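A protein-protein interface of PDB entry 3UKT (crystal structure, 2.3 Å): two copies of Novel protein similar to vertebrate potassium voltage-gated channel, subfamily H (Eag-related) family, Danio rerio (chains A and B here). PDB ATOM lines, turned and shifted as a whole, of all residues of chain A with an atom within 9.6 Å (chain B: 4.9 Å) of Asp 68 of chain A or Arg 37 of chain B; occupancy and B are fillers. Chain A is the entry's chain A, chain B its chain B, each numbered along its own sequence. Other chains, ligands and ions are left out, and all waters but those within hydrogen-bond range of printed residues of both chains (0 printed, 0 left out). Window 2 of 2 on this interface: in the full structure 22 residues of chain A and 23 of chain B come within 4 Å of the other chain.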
ATOM      1  N   LEU A  58      25.345  -7.515 -27.116  1.00  0.00           N
ATOM      2  CA  LEU A  58      24.040  -7.422 -27.774  1.00  0.00           C
ATOM      3  C   LEU A  58      23.747  -8.602 -28.685  1.00  0.00           C
ATOM      4  O   LEU A  58      22.708  -8.635 -29.366  1.00  0.00           O
ATOM      5  CB  LEU A  58      23.939  -6.116 -28.575  1.00  0.00           C
ATOM      6  CG  LEU A  58      24.291  -4.870 -27.755  1.00  0.00           C
ATOM      7  CD1 LEU A  58      24.327  -3.634 -28.617  1.00  0.00           C
ATOM      8  CD2 LEU A  58      23.314  -4.676 -26.575  1.00  0.00           C
ATOM      9  N   PHE A  61      20.188 -10.273 -28.127  1.00  0.00           N
ATOM     10  CA  PHE A  61      18.975  -9.491 -28.098  1.00  0.00           C
ATOM     11  C   PHE A  61      18.132  -9.847 -29.316  1.00  0.00           C
ATOM     12  O   PHE A  61      18.675 -10.253 -30.345  1.00  0.00           O
ATOM     13  CB  PHE A  61      19.317  -8.004 -28.086  1.00  0.00           C
ATOM     14  CG  PHE A  61      19.844  -7.518 -26.763  1.00  0.00           C
ATOM     15  CD1 PHE A  61      20.201  -8.408 -25.781  1.00  0.00           C
ATOM     16  CD2 PHE A  61      19.962  -6.168 -26.504  1.00  0.00           C
ATOM     17  CE1 PHE A  61      20.682  -7.966 -24.564  1.00  0.00           C
ATOM     18  CE2 PHE A  61      20.435  -5.727 -25.283  1.00  0.00           C
ATOM     19  CZ  PHE A  61      20.793  -6.628 -24.312  1.00  0.00           C
ATOM     20  N   PRO A  62      16.798  -9.718 -29.199  1.00  0.00           N
ATOM     21  CA  PRO A  62      15.882  -9.929 -30.331  1.00  0.00           C
ATOM     22  C   PRO A  62      16.231  -9.011 -31.494  1.00  0.00           C
ATOM     23  O   PRO A  62      16.783  -7.938 -31.249  1.00  0.00           O
ATOM     24  CB  PRO A  62      14.521  -9.523 -29.761  1.00  0.00           C
ATOM     25  CG  PRO A  62      14.645  -9.733 -28.294  1.00  0.00           C
ATOM     26  CD  PRO A  62      16.074  -9.410 -27.956  1.00  0.00           C
ATOM     27  N   ASP A  63      15.892  -9.418 -32.719  1.00  0.00           N
ATOM     28  CA  ASP A  63      16.247  -8.672 -33.922  1.00  0.00           C
ATOM     29  C   ASP A  63      15.701  -7.261 -33.899  1.00  0.00           C
ATOM     30  O   ASP A  63      16.335  -6.344 -34.411  1.00  0.00           O
ATOM     31  CB  ASP A  63      15.765  -9.387 -35.191  1.00  0.00           C
ATOM     32  CG  ASP A  63      16.566 -10.651 -35.498  1.00  0.00           C
ATOM     33  OD1 ASP A  63      17.791 -10.690 -35.223  1.00  0.00           O
ATOM     34  OD2 ASP A  63      15.973 -11.612 -36.032  1.00  0.00           O
ATOM     35  N   GLU A  64      14.527  -7.077 -33.304  1.00  0.00           N
ATOM     36  CA  GLU A  64      13.873  -5.765 -33.355  1.00  0.00           C
ATOM     37  C   GLU A  64      14.528  -4.791 -32.387  1.00  0.00           C
ATOM     38  O   GLU A  64      14.657  -3.600 -32.684  1.00  0.00           O
ATOM     39  CB  GLU A  64      12.361  -5.876 -33.094  1.00  0.00           C
ATOM     40  N   LEU A  65      14.948  -5.297 -31.231  1.00  0.00           N
ATOM     41  CA  LEU A  65      15.603  -4.446 -30.254  1.00  0.00           C
ATOM     42  C   LEU A  65      16.960  -4.033 -30.822  1.00  0.00           C
ATOM     43  O   LEU A  65      17.366  -2.869 -30.714  1.00  0.00           O
ATOM     44  CB  LEU A  65      15.721  -5.154 -28.898  1.00  0.00           C
ATOM     45  CG  LEU A  65      16.532  -4.468 -27.790  1.00  0.00           C
ATOM     46  CD1 LEU A  65      16.129  -3.014 -27.570  1.00  0.00           C
ATOM     47  CD2 LEU A  65      16.426  -5.245 -26.499  1.00  0.00           C
ATOM     48  N   ARG A  66      17.637  -4.979 -31.466  1.00  0.00           N
ATOM     49  CA  ARG A  66      18.903  -4.698 -32.130  1.00  0.00           C
ATOM     50  C   ARG A  66      18.744  -3.605 -33.203  1.00  0.00           C
ATOM     51  O   ARG A  66      19.532  -2.661 -33.264  1.00  0.00           O
ATOM     52  CB  ARG A  66      19.526  -5.984 -32.715  1.00  0.00           C
ATOM     53  CG  ARG A  66      20.057  -6.960 -31.652  1.00  0.00           C
ATOM     54  CD  ARG A  66      20.493  -8.312 -32.231  1.00  0.00           C
ATOM     55  NE  ARG A  66      21.400  -8.136 -33.364  1.00  0.00           N
ATOM     56  CZ  ARG A  66      22.720  -7.981 -33.254  1.00  0.00           C
ATOM     57  NH1 ARG A  66      23.295  -7.999 -32.054  1.00  0.00           N
ATOM     58  NH2 ARG A  66      23.475  -7.819 -34.343  1.00  0.00           N
ATOM     59  N   ALA A  67      17.717  -3.731 -34.038  1.00  0.00           N
ATOM     60  CA  ALA A  67      17.421  -2.716 -35.042  1.00  0.00           C
ATOM     61  C   ALA A  67      17.135  -1.359 -34.392  1.00  0.00           C
ATOM     62  O   ALA A  67      17.640  -0.328 -34.852  1.00  0.00           O
ATOM     63  CB  ALA A  67      16.256  -3.161 -35.933  1.00  0.00           C
ATOM     64  N   ASP A  68      16.352  -1.349 -33.315  1.00  0.00           N
ATOM     65  CA  ASP A  68      16.078  -0.089 -32.616  1.00  0.00           C
ATOM     66  C   ASP A  68      17.336   0.513 -32.007  1.00  0.00           C
ATOM     67  O   ASP A  68      17.456   1.735 -31.907  1.00  0.00           O
ATOM     68  CB  ASP A  68      15.008  -0.252 -31.533  1.00  0.00           C
ATOM     69  CG  ASP A  68      13.650  -0.620 -32.104  1.00  0.00           C
ATOM     70  OD1 ASP A  68      13.434  -0.393 -33.314  1.00  0.00           O
ATOM     71  OD2 ASP A  68      12.796  -1.136 -31.349  1.00  0.00           O
ATOM     72  N   ILE A  69      18.275  -0.331 -31.587  1.00  0.00           N
ATOM     73  CA  ILE A  69      19.520   0.209 -31.054  1.00  0.00           C
ATOM     74  C   ILE A  69      20.363   0.776 -32.187  1.00  0.00           C
ATOM     75  O   ILE A  69      20.915   1.874 -32.087  1.00  0.00           O
ATOM     76  CB  ILE A  69      20.349  -0.852 -30.287  1.00  0.00           C
ATOM     77  CG1 ILE A  69      19.662  -1.229 -28.976  1.00  0.00           C
ATOM     78  CG2 ILE A  69      21.745  -0.327 -29.995  1.00  0.00           C
ATOM     79  CD1 ILE A  69      20.065  -2.575 -28.458  1.00  0.00           C
ATOM     80  N   ALA A  70      20.468   0.023 -33.272  1.00  0.00           N
ATOM     81  CA  ALA A  70      21.317   0.444 -34.372  1.00  0.00           C
ATOM     82  C   ALA A  70      20.880   1.820 -34.924  1.00  0.00           C
ATOM     83  O   ALA A  70      21.715   2.691 -35.152  1.00  0.00           O
ATOM     84  CB  ALA A  70      21.331  -0.609 -35.441  1.00  0.00           C
ATOM     85  N   MET A  71      19.576   2.025 -35.089  1.00  0.00           N
ATOM     86  CA  MET A  71      19.041   3.306 -35.586  1.00  0.00           C
ATOM     87  C   MET A  71      19.495   4.534 -34.800  1.00  0.00           C
ATOM     88  O   MET A  71      19.371   5.645 -35.296  1.00  0.00           O
ATOM     89  CB  MET A  71      17.503   3.302 -35.609  1.00  0.00           C
ATOM     90  CG  MET A  71      16.878   2.394 -36.642  1.00  0.00           C
ATOM     91  SD  MET A  71      15.080   2.466 -36.597  1.00  0.00           S
ATOM     92  CE  MET A  71      14.635   0.751 -36.266  1.00  0.00           C
ATOM     93  N   HIS A  72      19.978   4.340 -33.573  1.00  0.00           N
ATOM     94  CA  HIS A  72      20.458   5.454 -32.746  1.00  0.00           C
ATOM     95  C   HIS A  72      21.954   5.637 -32.886  1.00  0.00           C
ATOM     96  O   HIS A  72      22.520   6.591 -32.352  1.00  0.00           O
ATOM     97  CB  HIS A  72      20.136   5.247 -31.266  1.00  0.00           C
ATOM     98  CG  HIS A  72      18.724   5.555 -30.908  1.00  0.00           C
ATOM     99  ND1 HIS A  72      17.666   4.765 -31.295  1.00  0.00           N
ATOM    100  CD2 HIS A  72      18.180   6.585 -30.205  1.00  0.00           C
ATOM    101  CE1 HIS A  72      16.534   5.280 -30.843  1.00  0.00           C
ATOM    102  NE2 HIS A  72      16.827   6.388 -30.177  1.00  0.00           N
ATOM    103  N   LEU A  73      22.601   4.701 -33.573  1.00  0.00           N
ATOM    104  CA  LEU A  73      24.020   4.829 -33.851  1.00  0.00           C
ATOM    105  C   LEU A  73      24.200   5.411 -35.248  1.00  0.00           C
ATOM    106  O   LEU A  73      23.431   5.110 -36.175  1.00  0.00           O
ATOM    107  CB  LEU A  73      24.732   3.475 -33.761  1.00  0.00           C
ATOM    108  CG  LEU A  73      24.547   2.639 -32.503  1.00  0.00           C
ATOM    109  CD1 LEU A  73      25.272   1.306 -32.631  1.00  0.00           C
ATOM    110  CD2 LEU A  73      25.013   3.382 -31.283  1.00  0.00           C
ATOM    111  N   ARG A  92      23.794  -2.393 -40.065  1.00  0.00           N
ATOM    112  CA  ARG A  92      23.259  -2.558 -38.715  1.00  0.00           C
ATOM    113  C   ARG A  92      24.144  -3.527 -37.938  1.00  0.00           C
ATOM    114  O   ARG A  92      24.576  -3.227 -36.814  1.00  0.00           O
ATOM    115  CB  ARG A  92      21.822  -3.085 -38.754  1.00  0.00           C
ATOM    116  N   SER A  95      27.384  -1.905 -37.244  1.00  0.00           N
ATOM    117  CA  SER A  95      27.336  -0.805 -36.304  1.00  0.00           C
ATOM    118  C   SER A  95      27.276  -1.353 -34.885  1.00  0.00           C
ATOM    119  O   SER A  95      27.836  -0.774 -33.953  1.00  0.00           O
ATOM    120  CB  SER A  95      26.165   0.134 -36.595  1.00  0.00           C
ATOM    121  OG  SER A  95      24.931  -0.518 -36.345  1.00  0.00           O
ATOM    122  N   LEU A  96      26.608  -2.482 -34.702  1.00  0.00           N
ATOM    123  CA  LEU A  96      26.419  -2.946 -33.331  1.00  0.00           C
ATOM    124  C   LEU A  96      27.693  -3.523 -32.693  1.00  0.00           C
ATOM    125  O   LEU A  96      27.699  -3.803 -31.479  1.00  0.00           O
ATOM    126  CB  LEU A  96      25.249  -3.923 -33.231  1.00  0.00           C
ATOM    127  CG  LEU A  96      23.867  -3.257 -33.292  1.00  0.00           C
ATOM    128  CD1 LEU A  96      22.780  -4.285 -33.263  1.00  0.00           C
ATOM    129  CD2 LEU A  96      23.704  -2.310 -32.140  1.00  0.00           C
ATOM    130  N   LYS B  32      15.527   6.535 -22.397  1.00  0.00           N
ATOM    131  CA  LYS B  32      15.167   5.686 -21.270  1.00  0.00           C
ATOM    132  C   LYS B  32      14.384   4.453 -21.693  1.00  0.00           C
ATOM    133  O   LYS B  32      14.659   3.346 -21.239  1.00  0.00           O
ATOM    134  CB  LYS B  32      14.354   6.470 -20.238  1.00  0.00           C
ATOM    135  CG  LYS B  32      15.176   7.350 -19.317  1.00  0.00           C
ATOM    136  CD  LYS B  32      14.361   7.809 -18.115  1.00  0.00           C
ATOM    137  N   ALA B  33      13.399   4.637 -22.558  1.00  0.00           N
ATOM    138  CA  ALA B  33      12.583   3.504 -22.971  1.00  0.00           C
ATOM    139  C   ALA B  33      13.398   2.390 -23.636  1.00  0.00           C
ATOM    140  O   ALA B  33      13.119   1.208 -23.410  1.00  0.00           O
ATOM    141  CB  ALA B  33      11.437   3.956 -23.877  1.00  0.00           C
ATOM    142  N   LEU B  34      14.389   2.763 -24.450  1.00  0.00           N
ATOM    143  CA  LEU B  34      15.227   1.778 -25.139  1.00  0.00           C
ATOM    144  C   LEU B  34      16.145   1.105 -24.126  1.00  0.00           C
ATOM    145  O   LEU B  34      16.211  -0.119 -24.044  1.00  0.00           O
ATOM    146  CB  LEU B  34      16.055   2.426 -26.258  1.00  0.00           C
ATOM    147  CG  LEU B  34      16.777   1.428 -27.176  1.00  0.00           C
ATOM    148  CD1 LEU B  34      15.774   0.487 -27.810  1.00  0.00           C
ATOM    149  CD2 LEU B  34      17.615   2.116 -28.267  1.00  0.00           C
ATOM    150  N   ALA B  35      16.845   1.929 -23.354  1.00  0.00           N
ATOM    151  CA  ALA B  35      17.602   1.465 -22.202  1.00  0.00           C
ATOM    152  C   ALA B  35      16.839   0.433 -21.372  1.00  0.00           C
ATOM    153  O   ALA B  35      17.348  -0.659 -21.086  1.00  0.00           O
ATOM    154  CB  ALA B  35      17.982   2.645 -21.335  1.00  0.00           C
ATOM    155  N   GLN B  36      15.615   0.776 -20.987  1.00  0.00           N
ATOM    156  CA  GLN B  36      14.827  -0.103 -20.129  1.00  0.00           C
ATOM    157  C   GLN B  36      14.564  -1.438 -20.818  1.00  0.00           C
ATOM    158  O   GLN B  36      14.677  -2.499 -20.198  1.00  0.00           O
ATOM    159  CB  GLN B  36      13.516   0.570 -19.705  1.00  0.00           C
ATOM    160  N   ARG B  37      14.218  -1.383 -22.101  1.00  0.00           N
ATOM    161  CA  ARG B  37      14.016  -2.605 -22.875  1.00  0.00           C
ATOM    162  C   ARG B  37      15.305  -3.418 -22.928  1.00  0.00           C
ATOM    163  O   ARG B  37      15.273  -4.650 -22.917  1.00  0.00           O
ATOM    164  CB  ARG B  37      13.588  -2.285 -24.299  1.00  0.00           C
ATOM    165  CG  ARG B  37      12.265  -1.544 -24.433  1.00  0.00           C
ATOM    166  CD  ARG B  37      12.051  -1.075 -25.878  1.00  0.00           C
ATOM    167  NE  ARG B  37      12.020  -2.187 -26.831  1.00  0.00           N
ATOM    168  CZ  ARG B  37      12.218  -2.059 -28.145  1.00  0.00           C
ATOM    169  NH1 ARG B  37      12.468  -0.866 -28.670  1.00  0.00           N
ATOM    170  NH2 ARG B  37      12.172  -3.121 -28.942  1.00  0.00           N
ATOM    171  N   MET B  38      16.436  -2.719 -22.989  1.00  0.00           N
ATOM    172  CA  MET B  38      17.737  -3.376 -23.131  1.00  0.00           C
ATOM    173  C   MET B  38      18.113  -4.069 -21.835  1.00  0.00           C
ATOM    174  O   MET B  38      18.509  -5.225 -21.838  1.00  0.00           O
ATOM    175  CB  MET B  38      18.833  -2.372 -23.511  1.00  0.00           C
ATOM    176  CG  MET B  38      18.668  -1.752 -24.892  1.00  0.00           C
ATOM    177  SD  MET B  38      19.861  -0.441 -25.219  1.00  0.00           S
ATOM    178  CE  MET B  38      21.408  -1.362 -25.086  1.00  0.00           C
ATOM    179  N   LEU B  39      17.997  -3.343 -20.733  1.00  0.00           N
ATOM    180  CA  LEU B  39      18.287  -3.889 -19.421  1.00  0.00           C
ATOM    181  C   LEU B  39      17.363  -5.056 -19.097  1.00  0.00           C
ATOM    182  O   LEU B  39      17.794  -6.047 -18.511  1.00  0.00           O
ATOM    183  CB  LEU B  39      18.190  -2.796 -18.360  1.00  0.00           C
ATOM    184  CG  LEU B  39      19.377  -1.826 -18.439  1.00  0.00           C
ATOM    185  CD1 LEU B  39      19.109  -0.516 -17.701  1.00  0.00           C
ATOM    186  CD2 LEU B  39      20.646  -2.478 -17.908  1.00  0.00           C
ATOM    187  N   GLU B  40      16.100  -4.939 -19.494  1.00  0.00           N
ATOM    188  CA  GLU B  40      15.119  -6.002 -19.293  1.00  0.00           C
ATOM    189  C   GLU B  40      15.527  -7.255 -20.041  1.00  0.00           C
ATOM    190  O   GLU B  40      15.472  -8.355 -19.497  1.00  0.00           O
ATOM    191  CB  GLU B  40      13.729  -5.561 -19.770  1.00  0.00           C
ATOM    192  CG  GLU B  40      12.902  -4.800 -18.724  1.00  0.00           C
ATOM    193  CD  GLU B  40      11.591  -4.214 -19.277  1.00  0.00           C
ATOM    194  OE1 GLU B  40      11.136  -4.620 -20.375  1.00  0.00           O
ATOM    195  OE2 GLU B  40      11.013  -3.334 -18.600  1.00  0.00           O
ATOM    196  N   CYS B  41      15.928  -7.085 -21.298  1.00  0.00           N
ATOM    197  CA  CYS B  41      16.280  -8.217 -22.139  1.00  0.00           C
ATOM    198  C   CYS B  41      17.577  -8.845 -21.626  1.00  0.00           C
ATOM    199  O   CYS B  41      17.775 -10.053 -21.688  1.00  0.00           O
ATOM    200  CB  CYS B  41      16.432  -7.763 -23.588  1.00  0.00           C
ATOM    201  SG  CYS B  41      16.999  -9.056 -24.735  1.00  0.00           S
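The backbone carbonyl oxygen (O) of Asp 68 of chain A is in hydrogen-bond range of a ring nitrogen (ND1) of His 72 of chain A.
Of the printed residues of chain B, Pro 62 of chain A touches Cys 41 (3.4 Å).
Of chain B, only Leu 34 (3.7 Å) and Arg 37 (2.7 Å) come within 4 Å of Asp 68 of chain A.
Of the printed residues of chain B, Ile 69 of chain A touches Leu 34 and Met 38.
No residue of chain A comes within 4 Å of Gln 36 of chain B.
Of chain A, only Leu 65 and Asp 68 come within 4 Å of Arg 37 of chain B.
Printed residues of chain A within 4 Å of Met 38 of chain B: Phe 61, Leu 65 and Ile 69.
No residue of chain A comes within 4 Å of Glu 40 of chain B.
No position is printed for both chains.
Of the 11 pairs that touch across the chains among the printed residues, none has its exchanged pair printed and touching as well.
CZ of Phe 61 of chain A touches O of Met 38 of chain B, at 3.6 Å.
Phe 61 of chain A touches Cys 41 of chain B.
Cys 41 of chain B touches Pro 62 of chain A.
Leu 65 of chain A touches Leu 34 of chain B.
O of Arg 37 of chain B touches CD2 of Leu 65 of chain A, 3.8 Å away.
Met 38 of chain B touches Leu 65 of chain A.
Leu 65 of chain A touches Cys 41 of chain B (CD2 to CB, 3.8 Å).
Leu 34 of chain B touches Asp 68 of chain A.
CA of Ile 69 of chain A touches CD2 of Leu 34 of chain B, 3.9 Å away.
CD1 of Ile 69 of chain A touches CE of Met 38 of chain B, 3.8 Å away.
Printed residues of chain A that touch a printed residue of chain B: Phe 61, Pro 62, Leu 65, Asp 68 and Ile 69.
Hydrophobic or aromatic side chains of chain A within 4 Å of the printed part of chain B: Phe 61, Pro 62, Leu 65 and Ile 69.
Of the 10 printed residues of chain B, 4 touch a printed residue of chain A.
The side-chain carboxylate (OD2) of Asp 68 of chain A lies within salt-bridge range of the guanidinium group (NH1) of Arg 37 of chain B, at 2.7 Å.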
